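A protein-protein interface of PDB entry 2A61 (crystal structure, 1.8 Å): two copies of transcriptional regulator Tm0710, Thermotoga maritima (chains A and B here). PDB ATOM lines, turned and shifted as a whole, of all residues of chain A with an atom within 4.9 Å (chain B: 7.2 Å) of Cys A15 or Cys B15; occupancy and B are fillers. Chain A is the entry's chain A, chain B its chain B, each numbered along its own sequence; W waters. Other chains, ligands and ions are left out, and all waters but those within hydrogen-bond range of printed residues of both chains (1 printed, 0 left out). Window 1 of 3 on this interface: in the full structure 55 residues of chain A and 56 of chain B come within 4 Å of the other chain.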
ATOM      1  N   LEU A  11      -8.055  21.366 -15.643  1.00  0.00           N
ATOM      2  CA  LEU A  11      -8.260  21.931 -14.296  1.00  0.00           C
ATOM      3  C   LEU A  11      -7.377  23.134 -14.035  1.00  0.00           C
ATOM      4  O   LEU A  11      -7.820  24.081 -13.387  1.00  0.00           O
ATOM      5  CB  LEU A  11      -8.067  20.925 -13.162  1.00  0.00           C
ATOM      6  CG  LEU A  11      -9.152  19.900 -12.900  1.00  0.00           C
ATOM      7  CD1 LEU A  11      -8.602  18.857 -11.890  1.00  0.00           C
ATOM      8  CD2 LEU A  11     -10.457  20.566 -12.408  1.00  0.00           C
ATOM      9  N   ARG A  12      -6.121  23.101 -14.508  1.00  0.00           N
ATOM     10  CA  ARG A  12      -5.235  24.252 -14.344  1.00  0.00           C
ATOM     11  C   ARG A  12      -5.842  25.535 -14.927  1.00  0.00           C
ATOM     12  O   ARG A  12      -5.785  26.616 -14.300  1.00  0.00           O
ATOM     13  CB  ARG A  12      -3.854  24.007 -14.955  1.00  0.00           C
ATOM     14  CG  ARG A  12      -2.787  24.918 -14.454  1.00  0.00           C
ATOM     15  CD  ARG A  12      -1.547  24.890 -15.358  1.00  0.00           C
ATOM     16  NE  ARG A  12      -1.112  23.512 -15.580  1.00  0.00           N
ATOM     17  CZ  ARG A  12      -0.568  23.054 -16.712  1.00  0.00           C
ATOM     18  NH1 ARG A  12      -0.374  23.862 -17.743  1.00  0.00           N
ATOM     19  NH2 ARG A  12      -0.213  21.778 -16.806  1.00  0.00           N
ATOM     20  N   GLU A  13      -6.409  25.430 -16.123  1.00  0.00           N
ATOM     21  CA  GLU A  13      -6.924  26.623 -16.784  1.00  0.00           C
ATOM     22  C   GLU A  13      -8.228  27.068 -16.107  1.00  0.00           C
ATOM     23  O   GLU A  13      -8.488  28.267 -15.995  1.00  0.00           O
ATOM     24  CB  GLU A  13      -7.126  26.365 -18.283  1.00  0.00           C
ATOM     25  CG  GLU A  13      -5.825  26.361 -19.146  1.00  0.00           C
ATOM     26  CD  GLU A  13      -6.069  25.693 -20.510  1.00  0.00           C
ATOM     27  OE1 GLU A  13      -6.532  24.518 -20.540  1.00  0.00           O
ATOM     28  OE2 GLU A  13      -5.834  26.364 -21.542  1.00  0.00           O
ATOM     29  N   ILE A  14      -9.035  26.099 -15.644  1.00  0.00           N
ATOM     30  CA  ILE A  14     -10.275  26.448 -14.931  1.00  0.00           C
ATOM     31  C   ILE A  14      -9.956  27.233 -13.656  1.00  0.00           C
ATOM     32  O   ILE A  14     -10.562  28.269 -13.386  1.00  0.00           O
ATOM     33  CB  ILE A  14     -11.096  25.174 -14.602  1.00  0.00           C
ATOM     34  CG1 ILE A  14     -11.752  24.645 -15.894  1.00  0.00           C
ATOM     35  CG2 ILE A  14     -12.146  25.446 -13.544  1.00  0.00           C
ATOM     36  CD1 ILE A  14     -12.286  23.195 -15.769  1.00  0.00           C
ATOM     37  N   CYS A  15      -9.020  26.696 -12.876  1.00  0.00           N
ATOM     38  CA  CYS A  15      -8.660  27.259 -11.578  1.00  0.00           C
ATOM     39  C   CYS A  15      -8.024  28.640 -11.743  1.00  0.00           C
ATOM     40  O   CYS A  15      -8.335  29.550 -10.973  1.00  0.00           O
ATOM     41  CB  CYS A  15      -7.727  26.326 -10.864  1.00  0.00           C
ATOM     42  SG  CYS A  15      -8.517  24.799 -10.446  1.00  0.00           S
ATOM     43  N   PHE A  16      -7.158  28.788 -12.756  1.00  0.00           N
ATOM     44  CA  PHE A  16      -6.537  30.061 -13.132  1.00  0.00           C
ATOM     45  C   PHE A  16      -7.593  31.116 -13.439  1.00  0.00           C
ATOM     46  O   PHE A  16      -7.515  32.214 -12.904  1.00  0.00           O
ATOM     47  CB  PHE A  16      -5.516  29.872 -14.294  1.00  0.00           C
ATOM     48  CG  PHE A  16      -4.900  31.169 -14.802  1.00  0.00           C
ATOM     49  CD1 PHE A  16      -3.773  31.711 -14.185  1.00  0.00           C
ATOM     50  CD2 PHE A  16      -5.462  31.850 -15.882  1.00  0.00           C
ATOM     51  CE1 PHE A  16      -3.201  32.906 -14.649  1.00  0.00           C
ATOM     52  CE2 PHE A  16      -4.900  33.046 -16.352  1.00  0.00           C
ATOM     53  CZ  PHE A  16      -3.778  33.576 -15.717  1.00  0.00           C
ATOM     54  N   MET A  17      -8.585  30.787 -14.278  1.00  0.00           N
ATOM     55  CA  MET A  17      -9.602  31.769 -14.680  1.00  0.00           C
ATOM     56  C   MET A  17     -10.452  32.244 -13.511  1.00  0.00           C
ATOM     57  O   MET A  17     -10.743  33.443 -13.395  1.00  0.00           O
ATOM     58  CB  MET A  17     -10.519  31.254 -15.817  1.00  0.00           C
ATOM     59  CG  MET A  17      -9.776  31.219 -17.174  1.00  0.00           C
ATOM     60  SD  MET A  17     -10.856  30.812 -18.553  1.00  0.00           S
ATOM     61  CE  MET A  17     -10.949  29.023 -18.318  1.00  0.00           C
ATOM     62  N   VAL A  18     -10.867  31.316 -12.653  1.00  0.00           N
ATOM     63  CA  VAL A  18     -11.665  31.753 -11.533  1.00  0.00           C
ATOM     64  C   VAL A  18     -10.806  32.539 -10.537  1.00  0.00           C
ATOM     65  O   VAL A  18     -11.309  33.460  -9.926  1.00  0.00           O
ATOM     66  CB  VAL A  18     -12.471  30.636 -10.886  1.00  0.00           C
ATOM     67  CG1 VAL A  18     -11.572  29.634 -10.289  1.00  0.00           C
ATOM     68  CG2 VAL A  18     -13.467  31.253  -9.863  1.00  0.00           C
ATOM     69  N   LYS A  19      -9.546  32.133 -10.355  1.00  0.00           N
ATOM     70  CA  LYS A  19      -8.621  32.867  -9.451  1.00  0.00           C
ATOM     71  C   LYS A  19      -8.460  34.322  -9.926  1.00  0.00           C
ATOM     72  O   LYS A  19      -8.625  35.262  -9.140  1.00  0.00           O
ATOM     73  CB  LYS A  19      -7.250  32.165  -9.389  1.00  0.00           C
ATOM     74  CG  LYS A  19      -6.173  32.855  -8.491  1.00  0.00           C
ATOM     75  CD  LYS A  19      -4.794  32.270  -8.809  1.00  0.00           C
ATOM     76  CE  LYS A  19      -3.667  32.877  -7.911  1.00  0.00           C
ATOM     77  NZ  LYS A  19      -3.882  32.368  -6.538  1.00  0.00           N
ATOM     78  N   ARG B   9     -17.954  26.958  -4.334  1.00  0.00           N
ATOM     79  CA  ARG B   9     -17.301  26.429  -3.167  1.00  0.00           C
ATOM     80  C   ARG B   9     -16.650  25.073  -3.457  1.00  0.00           C
ATOM     81  O   ARG B   9     -15.542  24.800  -3.015  1.00  0.00           O
ATOM     82  CB  ARG B   9     -18.319  26.288  -2.021  1.00  0.00           C
ATOM     83  CG  ARG B   9     -17.752  25.653  -0.760  1.00  0.00           C
ATOM     84  CD  ARG B   9     -16.817  26.620  -0.014  1.00  0.00           C
ATOM     85  NE  ARG B   9     -16.649  26.218   1.390  1.00  0.00           N
ATOM     86  CZ  ARG B   9     -15.563  25.612   1.864  1.00  0.00           C
ATOM     87  NH1 ARG B   9     -14.548  25.332   1.052  1.00  0.00           N
ATOM     88  NH2 ARG B   9     -15.484  25.289   3.151  1.00  0.00           N
ATOM     89  N   ILE B  10     -17.341  24.227  -4.205  1.00  0.00           N
ATOM     90  CA  ILE B  10     -16.832  22.900  -4.494  1.00  0.00           C
ATOM     91  C   ILE B  10     -15.645  23.020  -5.455  1.00  0.00           C
ATOM     92  O   ILE B  10     -14.640  22.360  -5.285  1.00  0.00           O
ATOM     93  CB  ILE B  10     -17.941  22.003  -5.075  1.00  0.00           C
ATOM     94  CG1 ILE B  10     -18.885  21.545  -3.936  1.00  0.00           C
ATOM     95  CG2 ILE B  10     -17.347  20.754  -5.746  1.00  0.00           C
ATOM     96  CD1 ILE B  10     -20.301  21.235  -4.412  1.00  0.00           C
ATOM     97  N   LEU B  11     -15.748  23.918  -6.429  1.00  0.00           N
ATOM     98  CA  LEU B  11     -14.639  24.114  -7.367  1.00  0.00           C
ATOM     99  C   LEU B  11     -13.433  24.766  -6.662  1.00  0.00           C
ATOM    100  O   LEU B  11     -12.273  24.420  -6.923  1.00  0.00           O
ATOM    101  CB  LEU B  11     -15.126  24.966  -8.541  1.00  0.00           C
ATOM    102  CG  LEU B  11     -14.150  25.142  -9.701  1.00  0.00           C
ATOM    103  CD1 LEU B  11     -13.979  23.770 -10.425  1.00  0.00           C
ATOM    104  CD2 LEU B  11     -14.587  26.277 -10.684  1.00  0.00           C
ATOM    105  N   ARG B  12     -13.699  25.681  -5.733  1.00  0.00           N
ATOM    106  CA  ARG B  12     -12.607  26.307  -4.946  1.00  0.00           C
ATOM    107  C   ARG B  12     -11.828  25.235  -4.170  1.00  0.00           C
ATOM    108  O   ARG B  12     -10.606  25.282  -4.074  1.00  0.00           O
ATOM    109  CB  ARG B  12     -13.152  27.347  -3.975  1.00  0.00           C
ATOM    110  CG  ARG B  12     -12.057  28.058  -3.122  1.00  0.00           C
ATOM    111  CD  ARG B  12     -12.591  28.583  -1.775  1.00  0.00           C
ATOM    112  NE  ARG B  12     -13.858  29.307  -1.909  1.00  0.00           N
ATOM    113  CZ  ARG B  12     -14.603  29.627  -0.879  1.00  0.00           C
ATOM    114  NH1 ARG B  12     -14.143  29.385   0.341  1.00  0.00           N
ATOM    115  NH2 ARG B  12     -15.777  30.226  -1.041  1.00  0.00           N
ATOM    116  N   GLU B  13     -12.549  24.261  -3.616  1.00  0.00           N
ATOM    117  CA  GLU B  13     -11.927  23.189  -2.841  1.00  0.00           C
ATOM    118  C   GLU B  13     -11.100  22.280  -3.728  1.00  0.00           C
ATOM    119  O   GLU B  13     -10.039  21.858  -3.323  1.00  0.00           O
ATOM    120  CB  GLU B  13     -12.986  22.402  -2.064  1.00  0.00           C
ATOM    121  CG  GLU B  13     -13.507  23.216  -0.887  1.00  0.00           C
ATOM    122  CD  GLU B  13     -12.394  23.465   0.153  1.00  0.00           C
ATOM    123  OE1 GLU B  13     -11.791  22.484   0.659  1.00  0.00           O
ATOM    124  OE2 GLU B  13     -12.092  24.635   0.436  1.00  0.00           O
ATOM    125  N   ILE B  14     -11.591  22.008  -4.938  1.00  0.00           N
ATOM    126  CA  ILE B  14     -10.867  21.171  -5.898  1.00  0.00           C
ATOM    127  C   ILE B  14      -9.556  21.895  -6.270  1.00  0.00           C
ATOM    128  O   ILE B  14      -8.484  21.296  -6.243  1.00  0.00           O
ATOM    129  CB  ILE B  14     -11.738  20.857  -7.163  1.00  0.00           C
ATOM    130  CG1 ILE B  14     -12.778  19.788  -6.846  1.00  0.00           C
ATOM    131  CG2 ILE B  14     -10.875  20.387  -8.359  1.00  0.00           C
ATOM    132  CD1 ILE B  14     -14.008  19.797  -7.743  1.00  0.00           C
ATOM    133  N   CYS B  15      -9.675  23.192  -6.549  1.00  0.00           N
ATOM    134  CA  CYS B  15      -8.558  24.034  -6.986  1.00  0.00           C
ATOM    135  C   CYS B  15      -7.506  24.138  -5.866  1.00  0.00           C
ATOM    136  O   CYS B  15      -6.317  24.009  -6.136  1.00  0.00           O
ATOM    137  CB  CYS B  15      -9.087  25.399  -7.469  1.00  0.00           C
ATOM    138  SG  CYS B  15      -9.965  25.315  -9.084  1.00  0.00           S
ATOM    139  N   PHE B  16      -7.949  24.325  -4.617  1.00  0.00           N
ATOM    140  CA  PHE B  16      -7.031  24.323  -3.444  1.00  0.00           C
ATOM    141  C   PHE B  16      -6.244  23.012  -3.294  1.00  0.00           C
ATOM    142  O   PHE B  16      -5.034  23.008  -3.081  1.00  0.00           O
ATOM    143  CB  PHE B  16      -7.794  24.675  -2.137  1.00  0.00           C
ATOM    144  CG  PHE B  16      -6.902  24.782  -0.923  1.00  0.00           C
ATOM    145  CD1 PHE B  16      -6.088  25.889  -0.743  1.00  0.00           C
ATOM    146  CD2 PHE B  16      -6.850  23.762   0.004  1.00  0.00           C
ATOM    147  CE1 PHE B  16      -5.260  26.004   0.356  1.00  0.00           C
ATOM    148  CE2 PHE B  16      -6.026  23.864   1.099  1.00  0.00           C
ATOM    149  CZ  PHE B  16      -5.233  25.006   1.278  1.00  0.00           C
ATOM    150  N   MET B  17      -6.943  21.888  -3.382  1.00  0.00           N
ATOM    151  CA  MET B  17      -6.305  20.584  -3.186  1.00  0.00           C
ATOM    152  C   MET B  17      -5.279  20.296  -4.264  1.00  0.00           C
ATOM    153  O   MET B  17      -4.201  19.765  -3.948  1.00  0.00           O
ATOM    154  CB  MET B  17      -7.353  19.443  -3.136  1.00  0.00           C
ATOM    155  CG  MET B  17      -8.065  19.365  -1.782  1.00  0.00           C
ATOM    156  SD  MET B  17      -9.135  17.935  -1.510  1.00  0.00           S
ATOM    157  CE  MET B  17     -10.584  18.475  -2.433  1.00  0.00           C
ATOM    158  N   VAL B  18      -5.627  20.584  -5.537  1.00  0.00           N
ATOM    159  CA  VAL B  18      -4.674  20.293  -6.636  1.00  0.00           C
ATOM    160  C   VAL B  18      -3.485  21.184  -6.522  1.00  0.00           C
ATOM    161  O   VAL B  18      -2.368  20.745  -6.740  1.00  0.00           O
ATOM    162  CB  VAL B  18      -5.332  20.277  -8.086  1.00  0.00           C
ATOM    163  CG1 VAL B  18      -5.805  21.673  -8.505  1.00  0.00           C
ATOM    164  CG2 VAL B  18      -4.393  19.637  -9.152  1.00  0.00           C
ATOM    165  N   LYS B  19      -3.701  22.436  -6.145  1.00  0.00           N
ATOM    166  CA  LYS B  19      -2.591  23.364  -5.956  1.00  0.00           C
ATOM    167  C   LYS B  19      -1.632  22.863  -4.861  1.00  0.00           C
ATOM    168  O   LYS B  19      -0.406  22.723  -5.060  1.00  0.00           O
ATOM    169  CB  LYS B  19      -3.098  24.762  -5.601  1.00  0.00           C
ATOM    170  CG  LYS B  19      -1.938  25.822  -5.499  1.00  0.00           C
ATOM    171  CD  LYS B  19      -2.442  27.148  -4.934  1.00  0.00           C
ATOM    172  CE  LYS B  19      -1.325  28.179  -5.004  1.00  0.00           C
ATOM    173  NZ  LYS B  19      -1.747  29.570  -4.655  1.00  0.00           N
ATOM    174  N   VAL B  20      -2.195  22.546  -3.700  1.00  0.00           N
ATOM    175  CA  VAL B  20      -1.356  22.139  -2.561  1.00  0.00           C
ATOM    176  C   VAL B  20      -0.670  20.813  -2.837  1.00  0.00           C
ATOM    177  O   VAL B  20       0.488  20.606  -2.467  1.00  0.00           O
ATOM    178  CB  VAL B  20      -2.191  22.087  -1.237  1.00  0.00           C
ATOM    179  CG1 VAL B  20      -1.448  21.305  -0.133  1.00  0.00           C
ATOM    180  CG2 VAL B  20      -2.548  23.544  -0.796  1.00  0.00           C
ATOM    181  N   GLU B  21      -1.392  19.908  -3.484  1.00  0.00           N
ATOM    182  CA  GLU B  21      -0.837  18.593  -3.818  1.00  0.00           C
ATOM    183  C   GLU B  21       0.456  18.735  -4.660  1.00  0.00           C
ATOM    184  O   GLU B  21       1.509  18.129  -4.339  1.00  0.00           O
ATOM    185  CB  GLU B  21      -1.892  17.769  -4.560  1.00  0.00           C
ATOM    186  CG  GLU B  21      -1.462  16.325  -4.855  1.00  0.00           C
ATOM    187  CD  GLU B  21      -1.269  15.555  -3.568  1.00  0.00           C
ATOM    188  OE1 GLU B  21      -1.968  15.903  -2.601  1.00  0.00           O
ATOM    189  OE2 GLU B  21      -0.428  14.643  -3.513  1.00  0.00           O
ATOM    190  N   ARG B 108       0.762  16.610  -9.744  1.00  0.00           N
ATOM    191  CA  ARG B 108      -0.648  16.922  -9.976  1.00  0.00           C
ATOM    192  C   ARG B 108      -1.322  15.887 -10.890  1.00  0.00           C
ATOM    193  O   ARG B 108      -2.421  15.408 -10.573  1.00  0.00           O
ATOM    194  CB  ARG B 108      -0.813  18.345 -10.535  1.00  0.00           C
ATOM    195  CG  ARG B 108      -0.417  19.481  -9.538  1.00  0.00           C
ATOM    196  CD  ARG B 108      -0.029  20.803 -10.284  1.00  0.00           C
ATOM    197  NE  ARG B 108      -1.065  21.265 -11.194  1.00  0.00           N
ATOM    198  CZ  ARG B 108      -2.058  22.087 -10.855  1.00  0.00           C
ATOM    199  NH1 ARG B 108      -2.107  22.586  -9.642  1.00  0.00           N
ATOM    200  NH2 ARG B 108      -2.965  22.473 -11.763  1.00  0.00           N
ATOM    201  N   MET B 138     -16.399  28.835 -19.589  1.00  0.00           N
ATOM    202  CA  MET B 138     -15.719  29.770 -18.684  1.00  0.00           C
ATOM    203  C   MET B 138     -14.850  30.773 -19.498  1.00  0.00           C
ATOM    204  O   MET B 138     -14.867  31.954 -19.238  1.00  0.00           O
ATOM    205  CB  MET B 138     -14.866  28.989 -17.690  1.00  0.00           C
ATOM    206  CG  MET B 138     -14.185  29.823 -16.627  1.00  0.00           C
ATOM    207  SD  MET B 138     -13.344  28.792 -15.392  1.00  0.00           S
ATOM    208  CE  MET B 138     -14.750  28.135 -14.521  1.00  0.00           C
HETATM  209  O   HOH W   1      -4.100  29.972  -5.835  1.00  0.00           O
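O of Ile A14 sits close to SD of Met B138, at 3.5 Å. SG of Cys B15 forms a disulfide with SG of Cys A15, at 2.1 Å.
The backbone carbonyl oxygen (O) of Val B18 is in hydrogen-bond range of the guanidinium group (NH1) of Arg B108 (3.4 Å).
Arg A12 touches Arg B108 (CG to NH2, 3.6 Å). CG2 of Ile A14 touches CD2 of Leu B11, at 3.9 Å. Met A17 touches Met B138. Lys A19 touches Lys B19.
Cys A15 touches just one residue of chain B: Cys B15. Of chain A, only Cys A15 comes within 4 Å of Cys B15. Of the printed residues of chain A, Met B138 touches Ile A14 and Met A17. Of the printed residues of chain A, Arg B108 touches Arg A12. Printed residues of chain A within 4 Å of Leu B11: Ile A14. Of the printed residues of chain B, Lys A19 touches Lys B19. Of the printed residues of chain A, Lys B19 touches Lys A19. The nearest residue of chain B that does not touch Cys A15 is Val B18 (4.6 Å).
Of the 9 printed residues of chain A, 5 touch a printed residue of chain B. Printed residues of chain A that touch a printed residue of chain B: Arg A12, Ile A14, Cys A15, Met A17 and Lys A19. Hydrophobic or aromatic side chains of chain A that line the printed part of chain B: Ile A14 and Met A17. Of the 15 printed residues of chain B, 5 touch a printed residue of chain A. Printed residues of chain B that touch a printed residue of chain A: Leu B11, Cys B15, Lys B19, Arg B108 and Met B138. Hydrophobic or aromatic side chains of chain B within 4 Å of the printed part of chain A: Leu B11 and Met B138. Among the printed residues, 6 pairs touch across the chains.
Ile A14 touches Leu B11, but with the chains exchanged Leu A11 does not touch Ile B14 (4.1 Å). Cys A15 touches its own counterpart, Cys B15. Lys A19 touches its own counterpart, Lys B19. Positions printed for both chains: 11, 12, 13, 14, 15, 16, 17, 18 and 19.
Water W1 lies within hydrogen-bond range of NZ of Lys A19 (2.5 Å) and NZ of Lys B19 (2.7 Å).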
